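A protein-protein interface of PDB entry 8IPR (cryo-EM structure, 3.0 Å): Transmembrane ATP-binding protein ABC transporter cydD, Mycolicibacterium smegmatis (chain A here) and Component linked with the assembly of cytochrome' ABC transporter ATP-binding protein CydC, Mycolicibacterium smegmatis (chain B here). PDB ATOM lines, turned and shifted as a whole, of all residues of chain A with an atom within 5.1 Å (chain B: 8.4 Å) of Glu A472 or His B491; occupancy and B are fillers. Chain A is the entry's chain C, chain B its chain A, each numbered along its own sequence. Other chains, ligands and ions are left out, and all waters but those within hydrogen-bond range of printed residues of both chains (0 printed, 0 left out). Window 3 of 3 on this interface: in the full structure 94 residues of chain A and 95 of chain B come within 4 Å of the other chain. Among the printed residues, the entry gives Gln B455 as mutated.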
ATOM      1  N   THR A 464     -10.102 -18.960  17.295  1.00  0.00           N
ATOM      2  CA  THR A 464      -8.741 -18.838  17.806  1.00  0.00           C
ATOM      3  C   THR A 464      -8.598 -17.714  18.827  1.00  0.00           C
ATOM      4  O   THR A 464      -7.544 -17.074  18.902  1.00  0.00           O
ATOM      5  CB  THR A 464      -7.756 -18.632  16.654  1.00  0.00           C
ATOM      6  OG1 THR A 464      -7.899 -17.306  16.132  1.00  0.00           O
ATOM      7  CG2 THR A 464      -8.013 -19.639  15.547  1.00  0.00           C
ATOM      8  N   LEU A 467      -5.655 -17.450  22.116  1.00  0.00           N
ATOM      9  CA  LEU A 467      -4.565 -18.322  21.703  1.00  0.00           C
ATOM     10  C   LEU A 467      -3.418 -17.493  21.142  1.00  0.00           C
ATOM     11  O   LEU A 467      -3.644 -16.490  20.456  1.00  0.00           O
ATOM     12  CB  LEU A 467      -5.036 -19.334  20.656  1.00  0.00           C
ATOM     13  CG  LEU A 467      -6.210 -20.235  21.042  1.00  0.00           C
ATOM     14  CD1 LEU A 467      -6.507 -21.227  19.934  1.00  0.00           C
ATOM     15  CD2 LEU A 467      -5.924 -20.959  22.343  1.00  0.00           C
ATOM     16  N   ASP A 468      -2.189 -17.912  21.435  1.00  0.00           N
ATOM     17  CA  ASP A 468      -1.006 -17.221  20.939  1.00  0.00           C
ATOM     18  C   ASP A 468      -0.777 -17.585  19.472  1.00  0.00           C
ATOM     19  O   ASP A 468      -1.582 -18.278  18.846  1.00  0.00           O
ATOM     20  CB  ASP A 468       0.206 -17.549  21.807  1.00  0.00           C
ATOM     21  CG  ASP A 468       0.343 -19.029  22.079  1.00  0.00           C
ATOM     22  OD1 ASP A 468      -0.570 -19.787  21.697  1.00  0.00           O
ATOM     23  OD2 ASP A 468       1.365 -19.439  22.665  1.00  0.00           O
ATOM     24  N   GLY A 469       0.341 -17.121  18.910  1.00  0.00           N
ATOM     25  CA  GLY A 469       0.573 -17.296  17.483  1.00  0.00           C
ATOM     26  C   GLY A 469       0.730 -18.746  17.064  1.00  0.00           C
ATOM     27  O   GLY A 469       0.148 -19.176  16.064  1.00  0.00           O
ATOM     28  N   ALA A 470       1.521 -19.518  17.812  1.00  0.00           N
ATOM     29  CA  ALA A 470       1.749 -20.914  17.448  1.00  0.00           C
ATOM     30  C   ALA A 470       0.464 -21.727  17.547  1.00  0.00           C
ATOM     31  O   ALA A 470       0.136 -22.507  16.643  1.00  0.00           O
ATOM     32  CB  ALA A 470       2.838 -21.515  18.336  1.00  0.00           C
ATOM     33  N   LEU A 471      -0.278 -21.555  18.642  1.00  0.00           N
ATOM     34  CA  LEU A 471      -1.547 -22.260  18.784  1.00  0.00           C
ATOM     35  C   LEU A 471      -2.553 -21.792  17.743  1.00  0.00           C
ATOM     36  O   LEU A 471      -3.339 -22.597  17.232  1.00  0.00           O
ATOM     37  CB  LEU A 471      -2.102 -22.072  20.193  1.00  0.00           C
ATOM     38  CG  LEU A 471      -1.732 -23.174  21.185  1.00  0.00           C
ATOM     39  CD1 LEU A 471      -1.870 -22.682  22.614  1.00  0.00           C
ATOM     40  CD2 LEU A 471      -2.583 -24.409  20.950  1.00  0.00           C
ATOM     41  N   GLU A 472      -2.549 -20.498  17.418  1.00  0.00           N
ATOM     42  CA  GLU A 472      -3.422 -20.002  16.360  1.00  0.00           C
ATOM     43  C   GLU A 472      -3.116 -20.694  15.038  1.00  0.00           C
ATOM     44  O   GLU A 472      -4.027 -21.131  14.327  1.00  0.00           O
ATOM     45  CB  GLU A 472      -3.271 -18.489  16.211  1.00  0.00           C
ATOM     46  CG  GLU A 472      -4.232 -17.671  17.052  1.00  0.00           C
ATOM     47  CD  GLU A 472      -4.075 -16.180  16.825  1.00  0.00           C
ATOM     48  OE1 GLU A 472      -4.006 -15.761  15.651  1.00  0.00           O
ATOM     49  OE2 GLU A 472      -4.016 -15.427  17.820  1.00  0.00           O
ATOM     50  N   ASP A 473      -1.830 -20.809  14.700  1.00  0.00           N
ATOM     51  CA  ASP A 473      -1.447 -21.465  13.456  1.00  0.00           C
ATOM     52  C   ASP A 473      -1.850 -22.932  13.456  1.00  0.00           C
ATOM     53  O   ASP A 473      -2.353 -23.443  12.450  1.00  0.00           O
ATOM     54  CB  ASP A 473       0.057 -21.321  13.228  1.00  0.00           C
ATOM     55  CG  ASP A 473       0.445 -19.929  12.774  1.00  0.00           C
ATOM     56  OD1 ASP A 473      -0.448 -19.177  12.331  1.00  0.00           O
ATOM     57  OD2 ASP A 473       1.643 -19.587  12.860  1.00  0.00           O
ATOM     58  N   ARG A 474      -1.641 -23.628  14.578  1.00  0.00           N
ATOM     59  CA  ARG A 474      -2.019 -25.038  14.648  1.00  0.00           C
ATOM     60  C   ARG A 474      -3.526 -25.221  14.504  1.00  0.00           C
ATOM     61  O   ARG A 474      -3.986 -26.115  13.782  1.00  0.00           O
ATOM     62  CB  ARG A 474      -1.523 -25.649  15.957  1.00  0.00           C
ATOM     63  CG  ARG A 474      -0.010 -25.704  16.075  1.00  0.00           C
ATOM     64  CD  ARG A 474       0.430 -26.419  17.340  1.00  0.00           C
ATOM     65  NE  ARG A 474      -0.121 -27.766  17.427  1.00  0.00           N
ATOM     66  CZ  ARG A 474      -0.091 -28.516  18.518  1.00  0.00           C
ATOM     67  NH1 ARG A 474       0.458 -28.081  19.641  1.00  0.00           N
ATOM     68  NH2 ARG A 474      -0.624 -29.734  18.484  1.00  0.00           N
ATOM     69  N   VAL A 475      -4.312 -24.379  15.177  1.00  0.00           N
ATOM     70  CA  VAL A 475      -5.764 -24.493  15.107  1.00  0.00           C
ATOM     71  C   VAL A 475      -6.262 -24.175  13.701  1.00  0.00           C
ATOM     72  O   VAL A 475      -7.160 -24.849  13.179  1.00  0.00           O
ATOM     73  CB  VAL A 475      -6.419 -23.585  16.164  1.00  0.00           C
ATOM     74  CG1 VAL A 475      -7.920 -23.510  15.950  1.00  0.00           C
ATOM     75  CG2 VAL A 475      -6.109 -24.097  17.559  1.00  0.00           C
ATOM     76  N   LEU A 476      -5.692 -23.151  13.064  1.00  0.00           N
ATOM     77  CA  LEU A 476      -6.096 -22.824  11.702  1.00  0.00           C
ATOM     78  C   LEU A 476      -5.702 -23.927  10.729  1.00  0.00           C
ATOM     79  O   LEU A 476      -6.441 -24.215   9.783  1.00  0.00           O
ATOM     80  CB  LEU A 476      -5.492 -21.485  11.278  1.00  0.00           C
ATOM     81  CG  LEU A 476      -6.023 -20.265  12.031  1.00  0.00           C
ATOM     82  CD1 LEU A 476      -5.116 -19.067  11.818  1.00  0.00           C
ATOM     83  CD2 LEU A 476      -7.446 -19.950  11.608  1.00  0.00           C
ATOM     84  N   ALA A 477      -4.549 -24.561  10.948  1.00  0.00           N
ATOM     85  CA  ALA A 477      -4.166 -25.700  10.120  1.00  0.00           C
ATOM     86  C   ALA A 477      -5.144 -26.854  10.288  1.00  0.00           C
ATOM     87  O   ALA A 477      -5.511 -27.513   9.310  1.00  0.00           O
ATOM     88  CB  ALA A 477      -2.744 -26.144  10.460  1.00  0.00           C
ATOM     89  N   ARG A 495      -9.243 -11.149  12.108  1.00  0.00           N
ATOM     90  CA  ARG A 495      -7.850 -10.794  12.329  1.00  0.00           C
ATOM     91  C   ARG A 495      -7.015 -11.297  11.160  1.00  0.00           C
ATOM     92  O   ARG A 495      -7.458 -12.132  10.369  1.00  0.00           O
ATOM     93  CB  ARG A 495      -7.318 -11.362  13.650  1.00  0.00           C
ATOM     94  CG  ARG A 495      -6.362 -10.428  14.367  1.00  0.00           C
ATOM     95  CD  ARG A 495      -6.263 -10.747  15.846  1.00  0.00           C
ATOM     96  NE  ARG A 495      -5.716  -9.622  16.596  1.00  0.00           N
ATOM     97  CZ  ARG A 495      -6.445  -8.763  17.294  1.00  0.00           C
ATOM     98  NH1 ARG A 495      -7.760  -8.880  17.380  1.00  0.00           N
ATOM     99  NH2 ARG A 495      -5.839  -7.759  17.922  1.00  0.00           N
ATOM    100  N   PRO A 497      -4.192 -13.277  10.747  1.00  0.00           N
ATOM    101  CA  PRO A 497      -3.965 -14.718  10.531  1.00  0.00           C
ATOM    102  C   PRO A 497      -5.218 -15.473  10.124  1.00  0.00           C
ATOM    103  O   PRO A 497      -5.141 -16.399   9.307  1.00  0.00           O
ATOM    104  CB  PRO A 497      -3.429 -15.193  11.889  1.00  0.00           C
ATOM    105  CG  PRO A 497      -2.860 -13.976  12.514  1.00  0.00           C
ATOM    106  CD  PRO A 497      -3.773 -12.869  12.100  1.00  0.00           C
ATOM    107  N   VAL B 339       2.853  -7.576  29.864  1.00  0.00           N
ATOM    108  CA  VAL B 339       3.022  -8.991  30.189  1.00  0.00           C
ATOM    109  C   VAL B 339       2.478  -9.859  29.061  1.00  0.00           C
ATOM    110  O   VAL B 339       1.305  -9.750  28.688  1.00  0.00           O
ATOM    111  CB  VAL B 339       2.328  -9.335  31.519  1.00  0.00           C
ATOM    112  CG1 VAL B 339       2.681 -10.748  31.952  1.00  0.00           C
ATOM    113  CG2 VAL B 339       2.708  -8.330  32.592  1.00  0.00           C
ATOM    114  N   VAL B 340       3.327 -10.724  28.508  1.00  0.00           N
ATOM    115  CA  VAL B 340       2.976 -11.582  27.388  1.00  0.00           C
ATOM    116  C   VAL B 340       3.454 -12.999  27.687  1.00  0.00           C
ATOM    117  O   VAL B 340       3.999 -13.282  28.752  1.00  0.00           O
ATOM    118  CB  VAL B 340       3.565 -11.072  26.055  1.00  0.00           C
ATOM    119  CG1 VAL B 340       2.741  -9.914  25.522  1.00  0.00           C
ATOM    120  CG2 VAL B 340       5.011 -10.655  26.240  1.00  0.00           C
ATOM    121  N   GLY B 341       3.234 -13.895  26.729  1.00  0.00           N
ATOM    122  CA  GLY B 341       3.648 -15.270  26.861  1.00  0.00           C
ATOM    123  C   GLY B 341       2.705 -16.224  26.161  1.00  0.00           C
ATOM    124  O   GLY B 341       1.741 -15.814  25.509  1.00  0.00           O
ATOM    125  N   SER B 343      -0.135 -19.511  25.932  1.00  0.00           N
ATOM    126  CA  SER B 343      -1.515 -19.591  26.394  1.00  0.00           C
ATOM    127  C   SER B 343      -1.678 -20.444  27.647  1.00  0.00           C
ATOM    128  O   SER B 343      -2.805 -20.830  27.978  1.00  0.00           O
ATOM    129  CB  SER B 343      -2.410 -20.126  25.275  1.00  0.00           C
ATOM    130  OG  SER B 343      -3.504 -20.852  25.801  1.00  0.00           O
ATOM    131  N   LYS B 347       0.014 -15.473  32.798  1.00  0.00           N
ATOM    132  CA  LYS B 347      -0.090 -14.017  32.789  1.00  0.00           C
ATOM    133  C   LYS B 347      -1.161 -13.523  33.754  1.00  0.00           C
ATOM    134  O   LYS B 347      -0.945 -12.545  34.479  1.00  0.00           O
ATOM    135  CB  LYS B 347      -0.375 -13.525  31.372  1.00  0.00           C
ATOM    136  CG  LYS B 347       0.597 -14.046  30.336  1.00  0.00           C
ATOM    137  CD  LYS B 347       0.231 -13.563  28.950  1.00  0.00           C
ATOM    138  CE  LYS B 347      -1.078 -14.166  28.493  1.00  0.00           C
ATOM    139  NZ  LYS B 347      -0.846 -15.406  27.712  1.00  0.00           N
ATOM    140  N   GLN B 455      -6.270  -9.321  28.824  1.00  0.00           N
ATOM    141  CA  GLN B 455      -6.689  -9.487  27.436  1.00  0.00           C
ATOM    142  C   GLN B 455      -7.810  -8.515  27.092  1.00  0.00           C
ATOM    143  O   GLN B 455      -8.939  -8.942  26.820  1.00  0.00           O
ATOM    144  CB  GLN B 455      -7.132 -10.927  27.178  1.00  0.00           C
ATOM    145  CG  GLN B 455      -6.017 -11.833  26.688  1.00  0.00           C
ATOM    146  CD  GLN B 455      -6.133 -13.243  27.227  1.00  0.00           C
ATOM    147  OE1 GLN B 455      -6.820 -14.086  26.651  1.00  0.00           O
ATOM    148  NE2 GLN B 455      -5.463 -13.507  28.342  1.00  0.00           N
ATOM    149  N   PRO B 456      -7.543  -7.205  27.090  1.00  0.00           N
ATOM    150  CA  PRO B 456      -8.630  -6.232  26.927  1.00  0.00           C
ATOM    151  C   PRO B 456      -9.069  -6.011  25.491  1.00  0.00           C
ATOM    152  O   PRO B 456     -10.125  -5.402  25.279  1.00  0.00           O
ATOM    153  CB  PRO B 456      -8.028  -4.952  27.513  1.00  0.00           C
ATOM    154  CG  PRO B 456      -6.565  -5.083  27.254  1.00  0.00           C
ATOM    155  CD  PRO B 456      -6.227  -6.552  27.190  1.00  0.00           C
ATOM    156  N   THR B 457      -8.309  -6.476  24.500  1.00  0.00           N
ATOM    157  CA  THR B 457      -8.647  -6.268  23.098  1.00  0.00           C
ATOM    158  C   THR B 457      -9.056  -7.565  22.408  1.00  0.00           C
ATOM    159  O   THR B 457      -8.809  -7.744  21.213  1.00  0.00           O
ATOM    160  CB  THR B 457      -7.485  -5.614  22.353  1.00  0.00           C
ATOM    161  OG1 THR B 457      -6.511  -6.608  22.015  1.00  0.00           O
ATOM    162  CG2 THR B 457      -6.836  -4.548  23.215  1.00  0.00           C
ATOM    163  N   GLU B 458      -9.680  -8.477  23.147  1.00  0.00           N
ATOM    164  CA  GLU B 458     -10.204  -9.705  22.571  1.00  0.00           C
ATOM    165  C   GLU B 458     -11.596  -9.462  22.004  1.00  0.00           C
ATOM    166  O   GLU B 458     -12.384  -8.700  22.570  1.00  0.00           O
ATOM    167  CB  GLU B 458     -10.253 -10.819  23.617  1.00  0.00           C
ATOM    168  CG  GLU B 458      -9.060 -11.755  23.579  1.00  0.00           C
ATOM    169  CD  GLU B 458      -9.006 -12.584  22.310  1.00  0.00           C
ATOM    170  OE1 GLU B 458     -10.069 -12.803  21.694  1.00  0.00           O
ATOM    171  OE2 GLU B 458      -7.898 -13.014  21.927  1.00  0.00           O
ATOM    172  N   ASN B 459     -11.884 -10.109  20.876  1.00  0.00           N
ATOM    173  CA  ASN B 459     -13.165 -10.003  20.177  1.00  0.00           C
ATOM    174  C   ASN B 459     -13.447  -8.590  19.684  1.00  0.00           C
ATOM    175  O   ASN B 459     -14.594  -8.261  19.371  1.00  0.00           O
ATOM    176  CB  ASN B 459     -14.328 -10.490  21.050  1.00  0.00           C
ATOM    177  CG  ASN B 459     -14.205 -11.948  21.431  1.00  0.00           C
ATOM    178  OD1 ASN B 459     -14.078 -12.818  20.571  1.00  0.00           O
ATOM    179  ND2 ASN B 459     -14.252 -12.227  22.727  1.00  0.00           N
ATOM    180  N   LEU B 460     -12.429  -7.740  19.601  1.00  0.00           N
ATOM    181  CA  LEU B 460     -12.625  -6.382  19.121  1.00  0.00           C
ATOM    182  C   LEU B 460     -12.456  -6.308  17.607  1.00  0.00           C
ATOM    183  O   LEU B 460     -12.059  -7.267  16.944  1.00  0.00           O
ATOM    184  CB  LEU B 460     -11.664  -5.410  19.806  1.00  0.00           C
ATOM    185  CG  LEU B 460     -11.952  -5.061  21.264  1.00  0.00           C
ATOM    186  CD1 LEU B 460     -11.074  -3.907  21.708  1.00  0.00           C
ATOM    187  CD2 LEU B 460     -13.415  -4.725  21.458  1.00  0.00           C
ATOM    188  N   ALA B 465      -8.904  -2.674  17.411  1.00  0.00           N
ATOM    189  CA  ALA B 465      -8.166  -3.423  18.425  1.00  0.00           C
ATOM    190  C   ALA B 465      -6.762  -2.864  18.621  1.00  0.00           C
ATOM    191  O   ALA B 465      -6.338  -2.608  19.754  1.00  0.00           O
ATOM    192  CB  ALA B 465      -8.105  -4.901  18.043  1.00  0.00           C
ATOM    193  N   ARG B 466      -6.023  -2.675  17.525  1.00  0.00           N
ATOM    194  CA  ARG B 466      -4.646  -2.204  17.636  1.00  0.00           C
ATOM    195  C   ARG B 466      -4.586  -0.799  18.218  1.00  0.00           C
ATOM    196  O   ARG B 466      -3.743  -0.509  19.075  1.00  0.00           O
ATOM    197  CB  ARG B 466      -3.966  -2.248  16.267  1.00  0.00           C
ATOM    198  CG  ARG B 466      -2.699  -1.421  16.177  1.00  0.00           C
ATOM    199  CD  ARG B 466      -1.852  -1.837  14.989  1.00  0.00           C
ATOM    200  NE  ARG B 466      -0.460  -1.432  15.143  1.00  0.00           N
ATOM    201  CZ  ARG B 466       0.541  -1.897  14.409  1.00  0.00           C
ATOM    202  NH1 ARG B 466       0.340  -2.789  13.452  1.00  0.00           N
ATOM    203  NH2 ARG B 466       1.774  -1.456  14.639  1.00  0.00           N
ATOM    204  N   LEU B 469      -5.335  -0.999  21.969  1.00  0.00           N
ATOM    205  CA  LEU B 469      -4.207  -1.531  22.727  1.00  0.00           C
ATOM    206  C   LEU B 469      -3.084  -0.508  22.840  1.00  0.00           C
ATOM    207  O   LEU B 469      -2.501  -0.326  23.918  1.00  0.00           O
ATOM    208  CB  LEU B 469      -3.700  -2.817  22.076  1.00  0.00           C
ATOM    209  CG  LEU B 469      -2.680  -3.630  22.873  1.00  0.00           C
ATOM    210  CD1 LEU B 469      -3.137  -3.805  24.309  1.00  0.00           C
ATOM    211  CD2 LEU B 469      -2.452  -4.976  22.215  1.00  0.00           C
ATOM    212  N   GLU B 470      -2.771   0.180  21.738  1.00  0.00           N
ATOM    213  CA  GLU B 470      -1.732   1.202  21.777  1.00  0.00           C
ATOM    214  C   GLU B 470      -2.116   2.338  22.714  1.00  0.00           C
ATOM    215  O   GLU B 470      -1.273   2.844  23.461  1.00  0.00           O
ATOM    216  CB  GLU B 470      -1.461   1.732  20.370  1.00  0.00           C
ATOM    217  CG  GLU B 470      -0.530   0.855  19.552  1.00  0.00           C
ATOM    218  CD  GLU B 470      -0.259   1.420  18.172  1.00  0.00           C
ATOM    219  OE1 GLU B 470      -1.094   2.204  17.675  1.00  0.00           O
ATOM    220  OE2 GLU B 470       0.789   1.080  17.587  1.00  0.00           O
ATOM    221  N   LEU B 473      -1.583   1.234  26.255  1.00  0.00           N
ATOM    222  CA  LEU B 473      -0.171   1.239  26.611  1.00  0.00           C
ATOM    223  C   LEU B 473       0.515   2.571  26.328  1.00  0.00           C
ATOM    224  O   LEU B 473       1.725   2.684  26.550  1.00  0.00           O
ATOM    225  CB  LEU B 473       0.558   0.108  25.882  1.00  0.00           C
ATOM    226  CG  LEU B 473       0.157  -1.293  26.353  1.00  0.00           C
ATOM    227  CD1 LEU B 473       0.947  -2.358  25.621  1.00  0.00           C
ATOM    228  CD2 LEU B 473       0.333  -1.427  27.856  1.00  0.00           C
ATOM    229  N   VAL B 487      -1.039  -4.656  31.232  1.00  0.00           N
ATOM    230  CA  VAL B 487      -1.898  -5.317  30.258  1.00  0.00           C
ATOM    231  C   VAL B 487      -1.278  -6.659  29.900  1.00  0.00           C
ATOM    232  O   VAL B 487      -0.141  -6.713  29.415  1.00  0.00           O
ATOM    233  CB  VAL B 487      -2.101  -4.457  29.001  1.00  0.00           C
ATOM    234  CG1 VAL B 487      -2.861  -5.235  27.944  1.00  0.00           C
ATOM    235  CG2 VAL B 487      -2.835  -3.176  29.350  1.00  0.00           C
ATOM    236  N   ALA B 488      -2.023  -7.736  30.137  1.00  0.00           N
ATOM    237  CA  ALA B 488      -1.648  -9.073  29.695  1.00  0.00           C
ATOM    238  C   ALA B 488      -2.353  -9.332  28.370  1.00  0.00           C
ATOM    239  O   ALA B 488      -3.582  -9.444  28.327  1.00  0.00           O
ATOM    240  CB  ALA B 488      -2.025 -10.123  30.737  1.00  0.00           C
ATOM    241  N   THR B 489      -1.580  -9.427  27.292  1.00  0.00           N
ATOM    242  CA  THR B 489      -2.147  -9.442  25.953  1.00  0.00           C
ATOM    243  C   THR B 489      -1.501 -10.535  25.116  1.00  0.00           C
ATOM    244  O   THR B 489      -0.416 -11.033  25.426  1.00  0.00           O
ATOM    245  CB  THR B 489      -1.982  -8.082  25.260  1.00  0.00           C
ATOM    246  OG1 THR B 489      -2.715  -8.077  24.029  1.00  0.00           O
ATOM    247  CG2 THR B 489      -0.517  -7.802  24.975  1.00  0.00           C
ATOM    248  N   HIS B 490      -2.200 -10.908  24.043  1.00  0.00           N
ATOM    249  CA  HIS B 490      -1.713 -11.878  23.075  1.00  0.00           C
ATOM    250  C   HIS B 490      -1.428 -11.277  21.707  1.00  0.00           C
ATOM    251  O   HIS B 490      -0.887 -11.977  20.846  1.00  0.00           O
ATOM    252  CB  HIS B 490      -2.730 -13.018  22.908  1.00  0.00           C
ATOM    253  CG  HIS B 490      -2.496 -14.182  23.816  1.00  0.00           C
ATOM    254  ND1 HIS B 490      -1.336 -14.926  23.789  1.00  0.00           N
ATOM    255  CD2 HIS B 490      -3.276 -14.738  24.772  1.00  0.00           C
ATOM    256  CE1 HIS B 490      -1.411 -15.886  24.692  1.00  0.00           C
ATOM    257  NE2 HIS B 490      -2.578 -15.794  25.303  1.00  0.00           N
ATOM    258  N   HIS B 491      -1.776 -10.012  21.484  1.00  0.00           N
ATOM    259  CA  HIS B 491      -1.677  -9.376  20.173  1.00  0.00           C
ATOM    260  C   HIS B 491      -0.883  -8.080  20.261  1.00  0.00           C
ATOM    261  O   HIS B 491      -1.277  -7.044  19.723  1.00  0.00           O
ATOM    262  CB  HIS B 491      -3.059  -9.106  19.590  1.00  0.00           C
ATOM    263  CG  HIS B 491      -4.019 -10.241  19.755  1.00  0.00           C
ATOM    264  ND1 HIS B 491      -3.778 -11.499  19.246  1.00  0.00           N
ATOM    265  CD2 HIS B 491      -5.224 -10.308  20.367  1.00  0.00           C
ATOM    266  CE1 HIS B 491      -4.792 -12.292  19.541  1.00  0.00           C
ATOM    267  NE2 HIS B 491      -5.683 -11.594  20.221  1.00  0.00           N
ATOM    268  N   LEU B 492       0.249  -8.121  20.947  1.00  0.00           N
ATOM    269  CA  LEU B 492       1.125  -6.957  20.989  1.00  0.00           C
ATOM    270  C   LEU B 492       1.737  -6.730  19.610  1.00  0.00           C
ATOM    271  O   LEU B 492       2.265  -7.675  19.011  1.00  0.00           O
ATOM    272  CB  LEU B 492       2.223  -7.146  22.031  1.00  0.00           C
ATOM    273  CG  LEU B 492       2.840  -5.860  22.585  1.00  0.00           C
ATOM    274  CD1 LEU B 492       1.775  -4.981  23.213  1.00  0.00           C
ATOM    275  CD2 LEU B 492       3.927  -6.185  23.590  1.00  0.00           C
ATOM    276  N   PRO B 493       1.672  -5.514  19.070  1.00  0.00           N
ATOM    277  CA  PRO B 493       2.218  -5.282  17.737  1.00  0.00           C
ATOM    278  C   PRO B 493       3.711  -5.536  17.716  1.00  0.00           C
ATOM    279  O   PRO B 493       4.416  -5.295  18.715  1.00  0.00           O
ATOM    280  CB  PRO B 493       1.893  -3.804  17.475  1.00  0.00           C
ATOM    281  CG  PRO B 493       0.768  -3.488  18.404  1.00  0.00           C
ATOM    282  CD  PRO B 493       1.024  -4.314  19.622  1.00  0.00           C
ATOM    283  N   PRO B 494       4.241  -6.044  16.598  1.00  0.00           N
ATOM    284  CA  PRO B 494       5.690  -6.313  16.535  1.00  0.00           C
ATOM    285  C   PRO B 494       6.544  -5.076  16.757  1.00  0.00           C
ATOM    286  O   PRO B 494       7.595  -5.162  17.404  1.00  0.00           O
ATOM    287  CB  PRO B 494       5.896  -6.897  15.129  1.00  0.00           C
ATOM    288  CG  PRO B 494       4.550  -7.070  14.527  1.00  0.00           C
ATOM    289  CD  PRO B 494       3.526  -6.380  15.356  1.00  0.00           C
ATOM    290  N   PHE B 496       6.615  -1.724  18.674  1.00  0.00           N
ATOM    291  CA  PHE B 496       5.955  -0.943  19.711  1.00  0.00           C
ATOM    292  C   PHE B 496       6.980  -0.623  20.800  1.00  0.00           C
ATOM    293  O   PHE B 496       8.190  -0.758  20.584  1.00  0.00           O
ATOM    294  CB  PHE B 496       4.722  -1.693  20.244  1.00  0.00           C
ATOM    295  CG  PHE B 496       3.738  -0.808  20.956  1.00  0.00           C
ATOM    296  CD1 PHE B 496       3.495   0.477  20.508  1.00  0.00           C
ATOM    297  CD2 PHE B 496       3.063  -1.260  22.076  1.00  0.00           C
ATOM    298  CE1 PHE B 496       2.596   1.294  21.160  1.00  0.00           C
ATOM    299  CE2 PHE B 496       2.162  -0.448  22.731  1.00  0.00           C
ATOM    300  CZ  PHE B 496       1.929   0.832  22.272  1.00  0.00           C
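NZ of Lys B347 sits at hydrogen-bond distance from NE2 of His B490. A ring nitrogen (NE2) of His B491 sits at hydrogen-bond distance from the side-chain carboxylate (OE2) of Glu B458 (3.1 Å). The backbone NH of His B491 lies within hydrogen-bond range of the side-chain hydroxyl of Thr B489 (3.3 Å).
Asp A468 touches Ser B343. CB of Asp A468 touches ND1 of His B490, 3.6 Å away. Leu A471 touches Ser B343 (CD1 to CB, 3.7 Å). His B491 touches Glu A472 (CE1 to OE2, 3.7 Å). Ala B465 touches Arg A495 (CB to NH2, 3.6 Å). Arg A495 touches His B491.
Ala A470 touches none of the printed residues of chain B. Printed residues of chain B within 4 Å of Leu A471: Ser B343. Glu A472 touches just one residue of chain B: His B491 (3.7 Å). Printed residues of chain A within 4 Å of Ser B343: Asp A468 (3.6 Å) and Leu A471 (3.7 Å). Of chain A, only Glu A472 (3.7 Å) and Arg A495 (3.5 Å) come within 4 Å of His B491.
Among the printed residues, no Asp or Glu carboxylate lies within 4 Å of a Lys or Arg side-chain nitrogen of the other chain.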
